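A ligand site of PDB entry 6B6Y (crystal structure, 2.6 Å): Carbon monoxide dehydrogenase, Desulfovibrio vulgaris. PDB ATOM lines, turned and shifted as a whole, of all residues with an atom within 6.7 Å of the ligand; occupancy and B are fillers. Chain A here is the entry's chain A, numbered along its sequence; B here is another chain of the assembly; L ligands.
The side-chain sulfur of Cys 67 is bound to an iron atom (FE2) of the ligand. N of Cys 82 sits close to S1 of the ligand (3.4 Å). SG of Cys 82 is bound to FE3 of the ligand (2.3 Å). The side-chain sulfur (SG) of Cys 59 binds an iron atom (FE1) of the ligand (2.3 Å). The side-chain sulfur (SG) of Cys 62 binds an iron atom (FE4) of the ligand (2.3 Å). NH2 of Arg 92 lies close to S4 of the ligand (3.5 Å).
O of Cys 67 sits at hydrogen-bond distance from N of Cys 59 (3.0 Å). The backbone NH of Val 81 lies close to the side-chain sulfur of Cys 67, at 3.5 Å. SG of Cys 59 sits close to NH2 of Arg 92 (3.4 Å). N of Asn 61 sits close to SG of Cys 59 (3.8 Å). The side-chain sulfur of Cys 62 lies close to the backbone NH of Met 64 (3.5 Å). ND2 of Asn 61 is in hydrogen-bond range of O of Thr 209, 2.7 Å away.
Merely in contact with the ligand: Met 64 (3.6 Å), Met 211 (3.6 Å), Ile 89 (3.7 Å), Gly 65 (3.8 Å), Val 81 (3.9 Å), Gly 80 (3.96 Å) and Asn 61 (3.97 Å). Hydrophobic or aromatic side chains that line the ligand: Met 64, Val 81, Ile 89 and Met 211. Along chain A the residues within 4 Å of the ligand span positions 59 to 211.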
ATOM      1  N   THR A  58      18.117   9.387  19.872  1.00  0.00           N
ATOM      2  CA  THR A  58      18.949  10.061  18.886  1.00  0.00           C
ATOM      3  C   THR A  58      18.690   9.435  17.526  1.00  0.00           C
ATOM      4  O   THR A  58      18.453   8.231  17.428  1.00  0.00           O
ATOM      5  CB  THR A  58      20.434   9.934  19.262  1.00  0.00           C
ATOM      6  OG1 THR A  58      21.253  10.460  18.211  1.00  0.00           O
ATOM      7  CG2 THR A  58      20.801   8.469  19.509  1.00  0.00           C
ATOM      8  N   CYS A  59      18.705  10.257  16.483  1.00  0.00           N
ATOM      9  CA  CYS A  59      18.386   9.792  15.133  1.00  0.00           C
ATOM     10  C   CYS A  59      19.317  10.455  14.136  1.00  0.00           C
ATOM     11  O   CYS A  59      19.467  11.678  14.138  1.00  0.00           O
ATOM     12  CB  CYS A  59      16.918  10.087  14.791  1.00  0.00           C
ATOM     13  SG  CYS A  59      16.313   9.400  13.222  1.00  0.00           S
ATOM     14  N   ARG A  60      19.958   9.632  13.293  1.00  0.00           N
ATOM     15  CA  ARG A  60      20.875  10.096  12.262  1.00  0.00           C
ATOM     16  C   ARG A  60      20.439   9.603  10.885  1.00  0.00           C
ATOM     17  O   ARG A  60      21.265   9.475   9.971  1.00  0.00           O
ATOM     18  CB  ARG A  60      22.311   9.682  12.568  1.00  0.00           C
ATOM     19  CG  ARG A  60      22.797  10.044  13.970  1.00  0.00           C
ATOM     20  N   ASN A  61      19.137   9.324  10.720  1.00  0.00           N
ATOM     21  CA  ASN A  61      18.602   8.710   9.497  1.00  0.00           C
ATOM     22  C   ASN A  61      18.507   9.662   8.319  1.00  0.00           C
ATOM     23  O   ASN A  61      18.191   9.212   7.214  1.00  0.00           O
ATOM     24  CB  ASN A  61      17.238   8.061   9.758  1.00  0.00           C
ATOM     25  CG  ASN A  61      17.349   6.746  10.518  1.00  0.00           C
ATOM     26  OD1 ASN A  61      18.402   6.414  11.074  1.00  0.00           O
ATOM     27  ND2 ASN A  61      16.261   5.980  10.537  1.00  0.00           N
ATOM     28  N   CYS A  62      18.766  10.954   8.519  1.00  0.00           N
ATOM     29  CA  CYS A  62      18.834  11.913   7.421  1.00  0.00           C
ATOM     30  C   CYS A  62      19.619  13.130   7.896  1.00  0.00           C
ATOM     31  O   CYS A  62      19.910  13.287   9.075  1.00  0.00           O
ATOM     32  CB  CYS A  62      17.420  12.286   6.916  1.00  0.00           C
ATOM     33  SG  CYS A  62      16.536  13.532   7.881  1.00  0.00           S
ATOM     34  N   ILE A  63      19.995  13.984   6.937  1.00  0.00           N
ATOM     35  CA  ILE A  63      20.804  15.155   7.239  1.00  0.00           C
ATOM     36  C   ILE A  63      19.962  16.406   7.462  1.00  0.00           C
ATOM     37  O   ILE A  63      20.512  17.507   7.611  1.00  0.00           O
ATOM     38  CB  ILE A  63      21.959  15.386   6.265  1.00  0.00           C
ATOM     39  CG1 ILE A  63      21.455  15.865   4.910  1.00  0.00           C
ATOM     40  CG2 ILE A  63      22.799  14.121   6.141  1.00  0.00           C
ATOM     41  CD1 ILE A  63      22.472  16.677   4.145  1.00  0.00           C
ATOM     42  N   MET A  64      18.636  16.278   7.480  1.00  0.00           N
ATOM     43  CA  MET A  64      17.832  17.295   8.169  1.00  0.00           C
ATOM     44  C   MET A  64      18.214  17.330   9.637  1.00  0.00           C
ATOM     45  O   MET A  64      18.273  18.410  10.238  1.00  0.00           O
ATOM     46  CB  MET A  64      16.339  17.013   8.005  1.00  0.00           C
ATOM     47  CG  MET A  64      15.778  17.309   6.627  1.00  0.00           C
ATOM     48  SD  MET A  64      13.994  17.624   6.694  1.00  0.00           S
ATOM     49  CE  MET A  64      13.421  16.160   7.541  1.00  0.00           C
ATOM     50  N   GLY A  65      18.512  16.170  10.215  1.00  0.00           N
ATOM     51  CA  GLY A  65      19.034  16.075  11.556  1.00  0.00           C
ATOM     52  C   GLY A  65      20.538  16.268  11.573  1.00  0.00           C
ATOM     53  O   GLY A  65      21.109  16.931  10.711  1.00  0.00           O
ATOM     54  N   PRO A  66      21.221  15.646  12.556  1.00  0.00           N
ATOM     55  CA  PRO A  66      20.697  14.708  13.547  1.00  0.00           C
ATOM     56  C   PRO A  66      19.818  15.364  14.606  1.00  0.00           C
ATOM     57  O   PRO A  66      19.936  16.568  14.858  1.00  0.00           O
ATOM     58  CB  PRO A  66      21.972  14.170  14.202  1.00  0.00           C
ATOM     59  CG  PRO A  66      22.932  15.304  14.101  1.00  0.00           C
ATOM     60  CD  PRO A  66      22.651  15.930  12.765  1.00  0.00           C
ATOM     61  N   CYS A  67      18.933  14.563  15.219  1.00  0.00           N
ATOM     62  CA  CYS A  67      17.948  15.045  16.163  1.00  0.00           C
ATOM     63  C   CYS A  67      18.063  14.282  17.467  1.00  0.00           C
ATOM     64  O   CYS A  67      18.298  13.074  17.473  1.00  0.00           O
ATOM     65  CB  CYS A  67      16.525  14.858  15.615  1.00  0.00           C
ATOM     66  SG  CYS A  67      16.223  15.595  13.979  1.00  0.00           S
ATOM     67  N   ARG A  68      17.904  15.009  18.573  1.00  0.00           N
ATOM     68  CA  ARG A  68      17.820  14.426  19.908  1.00  0.00           C
ATOM     69  C   ARG A  68      16.489  14.845  20.521  1.00  0.00           C
ATOM     70  O   ARG A  68      16.081  16.009  20.404  1.00  0.00           O
ATOM     71  CB  ARG A  68      18.956  14.935  20.802  1.00  0.00           C
ATOM     72  CG  ARG A  68      20.354  14.733  20.257  1.00  0.00           C
ATOM     73  CD  ARG A  68      21.371  15.558  21.033  1.00  0.00           C
ATOM     74  N   ILE A  69      15.828  13.919  21.173  1.00  0.00           N
ATOM     75  CA  ILE A  69      14.568  14.205  21.846  1.00  0.00           C
ATOM     76  C   ILE A  69      14.845  14.537  23.294  1.00  0.00           C
ATOM     77  O   ILE A  69      15.666  13.885  23.956  1.00  0.00           O
ATOM     78  CB  ILE A  69      13.582  13.026  21.711  1.00  0.00           C
ATOM     79  CG1 ILE A  69      13.351  12.694  20.233  1.00  0.00           C
ATOM     80  CG2 ILE A  69      12.251  13.359  22.368  1.00  0.00           C
ATOM     81  CD1 ILE A  69      12.861  13.873  19.437  1.00  0.00           C
ATOM     82  N   LEU A  79      10.217  16.722  19.416  1.00  0.00           N
ATOM     83  CA  LEU A  79      10.067  16.030  18.147  1.00  0.00           C
ATOM     84  C   LEU A  79      11.310  16.234  17.296  1.00  0.00           C
ATOM     85  O   LEU A  79      12.106  17.152  17.522  1.00  0.00           O
ATOM     86  CB  LEU A  79       8.867  16.586  17.379  1.00  0.00           C
ATOM     87  CG  LEU A  79       7.547  16.595  18.144  1.00  0.00           C
ATOM     88  CD1 LEU A  79       6.469  17.256  17.313  1.00  0.00           C
ATOM     89  CD2 LEU A  79       7.163  15.165  18.480  1.00  0.00           C
ATOM     90  N   GLY A  80      11.476  15.352  16.298  1.00  0.00           N
ATOM     91  CA  GLY A  80      12.481  15.548  15.287  1.00  0.00           C
ATOM     92  C   GLY A  80      12.081  16.631  14.298  1.00  0.00           C
ATOM     93  O   GLY A  80      10.970  17.152  14.329  1.00  0.00           O
ATOM     94  N   VAL A  81      13.029  16.979  13.420  1.00  0.00           N
ATOM     95  CA  VAL A  81      12.739  18.010  12.425  1.00  0.00           C
ATOM     96  C   VAL A  81      11.609  17.566  11.496  1.00  0.00           C
ATOM     97  O   VAL A  81      10.780  18.381  11.072  1.00  0.00           O
ATOM     98  CB  VAL A  81      14.028  18.399  11.662  1.00  0.00           C
ATOM     99  CG1 VAL A  81      13.748  19.482  10.643  1.00  0.00           C
ATOM    100  CG2 VAL A  81      15.097  18.869  12.634  1.00  0.00           C
ATOM    101  N   CYS A  82      11.535  16.265  11.206  1.00  0.00           N
ATOM    102  CA  CYS A  82      10.446  15.729  10.393  1.00  0.00           C
ATOM    103  C   CYS A  82       9.145  15.586  11.186  1.00  0.00           C
ATOM    104  O   CYS A  82       8.119  15.248  10.596  1.00  0.00           O
ATOM    105  CB  CYS A  82      10.843  14.390   9.782  1.00  0.00           C
ATOM    106  SG  CYS A  82      11.206  13.055  10.964  1.00  0.00           S
ATOM    107  N   GLY A  83       9.167  15.835  12.493  1.00  0.00           N
ATOM    108  CA  GLY A  83       8.002  15.670  13.323  1.00  0.00           C
ATOM    109  C   GLY A  83       7.948  14.385  14.114  1.00  0.00           C
ATOM    110  O   GLY A  83       6.968  14.160  14.841  1.00  0.00           O
ATOM    111  N   ALA A  84       8.966  13.530  14.017  1.00  0.00           N
ATOM    112  CA  ALA A  84       8.963  12.242  14.705  1.00  0.00           C
ATOM    113  C   ALA A  84       9.179  12.415  16.202  1.00  0.00           C
ATOM    114  O   ALA A  84      10.051  13.175  16.635  1.00  0.00           O
ATOM    115  CB  ALA A  84      10.046  11.336  14.120  1.00  0.00           C
ATOM    116  N   ILE A  89      11.220   7.351  16.913  1.00  0.00           N
ATOM    117  CA  ILE A  89      12.682   7.375  16.824  1.00  0.00           C
ATOM    118  C   ILE A  89      13.285   6.174  17.542  1.00  0.00           C
ATOM    119  O   ILE A  89      14.176   5.497  17.009  1.00  0.00           O
ATOM    120  CB  ILE A  89      13.232   8.714  17.353  1.00  0.00           C
ATOM    121  CG1 ILE A  89      12.905   9.848  16.375  1.00  0.00           C
ATOM    122  CG2 ILE A  89      14.726   8.630  17.608  1.00  0.00           C
ATOM    123  CD1 ILE A  89      13.325  11.212  16.860  1.00  0.00           C
ATOM    124  N   ARG A  92      12.460   2.936  15.623  1.00  0.00           N
ATOM    125  CA  ARG A  92      13.231   2.806  14.389  1.00  0.00           C
ATOM    126  C   ARG A  92      14.641   2.281  14.682  1.00  0.00           C
ATOM    127  O   ARG A  92      15.089   1.316  14.053  1.00  0.00           O
ATOM    128  CB  ARG A  92      13.276   4.141  13.647  1.00  0.00           C
ATOM    129  CG  ARG A  92      11.955   4.503  12.999  1.00  0.00           C
ATOM    130  CD  ARG A  92      12.039   5.728  12.098  1.00  0.00           C
ATOM    131  NE  ARG A  92      12.518   6.921  12.781  1.00  0.00           N
ATOM    132  CZ  ARG A  92      12.487   8.141  12.237  1.00  0.00           C
ATOM    133  NH1 ARG A  92      12.013   8.306  11.015  1.00  0.00           N
ATOM    134  NH2 ARG A  92      12.947   9.191  12.914  1.00  0.00           N
ATOM    135  N   THR A 209      12.326   2.125   8.272  1.00  0.00           N
ATOM    136  CA  THR A 209      13.029   3.086   9.121  1.00  0.00           C
ATOM    137  C   THR A 209      13.581   4.293   8.371  1.00  0.00           C
ATOM    138  O   THR A 209      14.199   5.155   9.000  1.00  0.00           O
ATOM    139  CB  THR A 209      14.125   2.391   9.936  1.00  0.00           C
ATOM    140  OG1 THR A 209      14.890   1.520   9.087  1.00  0.00           O
ATOM    141  CG2 THR A 209      13.510   1.570  11.037  1.00  0.00           C
ATOM    142  N   HIS A 210      13.383   4.381   7.055  1.00  0.00           N
ATOM    143  CA  HIS A 210      13.712   5.593   6.324  1.00  0.00           C
ATOM    144  C   HIS A 210      12.743   6.708   6.725  1.00  0.00           C
ATOM    145  O   HIS A 210      11.600   6.450   7.139  1.00  0.00           O
ATOM    146  CB  HIS A 210      13.601   5.337   4.812  1.00  0.00           C
ATOM    147  CG  HIS A 210      14.089   6.477   3.959  1.00  0.00           C
ATOM    148  ND1 HIS A 210      13.350   7.613   3.730  1.00  0.00           N
ATOM    149  CD2 HIS A 210      15.243   6.627   3.263  1.00  0.00           C
ATOM    150  CE1 HIS A 210      14.028   8.429   2.941  1.00  0.00           C
ATOM    151  NE2 HIS A 210      15.184   7.856   2.650  1.00  0.00           N
ATOM    152  N   MET A 211      13.216   7.952   6.641  1.00  0.00           N
ATOM    153  CA  MET A 211      12.399   9.116   6.980  1.00  0.00           C
ATOM    154  C   MET A 211      11.059   9.063   6.252  1.00  0.00           C
ATOM    155  O   MET A 211      10.999   8.766   5.051  1.00  0.00           O
ATOM    156  CB  MET A 211      13.134  10.406   6.591  1.00  0.00           C
ATOM    157  CG  MET A 211      12.530  11.700   7.178  1.00  0.00           C
ATOM    158  SD  MET A 211      10.941  12.239   6.490  1.00  0.00           S
ATOM    159  CE  MET A 211      11.343  13.840   5.788  1.00  0.00           C
ATOM    160  N   GLY A 212       9.987   9.344   6.995  1.00  0.00           N
ATOM    161  CA  GLY A 212       8.683   9.506   6.393  1.00  0.00           C
ATOM    162  C   GLY A 212       8.054   8.240   5.869  1.00  0.00           C
ATOM    163  O   GLY A 212       7.246   8.298   4.937  1.00  0.00           O
ATOM    164  N   GLN B  46      16.814  21.870  16.772  1.00  0.00           N
ATOM    165  CA  GLN B  46      17.871  20.871  16.697  1.00  0.00           C
ATOM    166  C   GLN B  46      19.205  21.434  16.232  1.00  0.00           C
ATOM    167  O   GLN B  46      20.104  20.660  15.887  1.00  0.00           O
ATOM    168  CB  GLN B  46      17.440  19.712  15.804  1.00  0.00           C
ATOM    169  CG  GLN B  46      16.219  18.948  16.306  1.00  0.00           C
ATOM    170  CD  GLN B  46      16.529  18.110  17.538  1.00  0.00           C
ATOM    171  OE1 GLN B  46      17.687  17.895  17.881  1.00  0.00           O
ATOM    172  NE2 GLN B  46      15.477  17.652  18.215  1.00  0.00           N
ATOM    173  N   PRO B 351       5.804  12.930   9.371  1.00  0.00           N
ATOM    174  CA  PRO B 351       4.710  12.621  10.304  1.00  0.00           C
ATOM    175  C   PRO B 351       4.050  13.856  10.892  1.00  0.00           C
ATOM    176  O   PRO B 351       2.940  13.739  11.421  1.00  0.00           O
ATOM    177  CB  PRO B 351       5.383  11.778  11.386  1.00  0.00           C
ATOM    178  CG  PRO B 351       6.844  12.098  11.275  1.00  0.00           C
ATOM    179  CD  PRO B 351       7.085  12.361   9.815  1.00  0.00           C
ATOM    180  N   TYR B 561      18.787  15.785   1.516  1.00  0.00           N
ATOM    181  CA  TYR B 561      18.630  15.469   2.940  1.00  0.00           C
ATOM    182  C   TYR B 561      18.516  13.977   3.243  1.00  0.00           C
ATOM    183  O   TYR B 561      18.913  13.563   4.339  1.00  0.00           O
ATOM    184  CB  TYR B 561      17.420  16.192   3.553  1.00  0.00           C
ATOM    185  CG  TYR B 561      16.133  15.400   3.444  1.00  0.00           C
ATOM    186  CD1 TYR B 561      15.369  15.433   2.280  1.00  0.00           C
ATOM    187  CD2 TYR B 561      15.679  14.598   4.489  1.00  0.00           C
ATOM    188  CE1 TYR B 561      14.206  14.700   2.162  1.00  0.00           C
ATOM    189  CE2 TYR B 561      14.525  13.856   4.376  1.00  0.00           C
ATOM    190  CZ  TYR B 561      13.783  13.915   3.218  1.00  0.00           C
ATOM    191  OH  TYR B 561      12.626  13.183   3.108  1.00  0.00           O
HETATM  192 FE1  LIG L   1      15.579  11.275  12.141  1.00  0.00          FE
HETATM  193 FE2  LIG L   1      15.592  13.983  12.517  1.00  0.00          FE
HETATM  194 FE3  LIG L   1      13.443  12.772  11.308  1.00  0.00          FE
HETATM  195 FE4  LIG L   1      15.832  12.951   9.980  1.00  0.00          FE
HETATM  196  S1  LIG L   1      14.497  14.686  10.640  1.00  0.00           S
HETATM  197  S2  LIG L   1      14.479  11.106  10.144  1.00  0.00           S
HETATM  198  S3  LIG L   1      17.306  12.709  11.705  1.00  0.00           S
HETATM  199  S4  LIG L   1      14.166  12.471  13.455  1.00  0.00           S
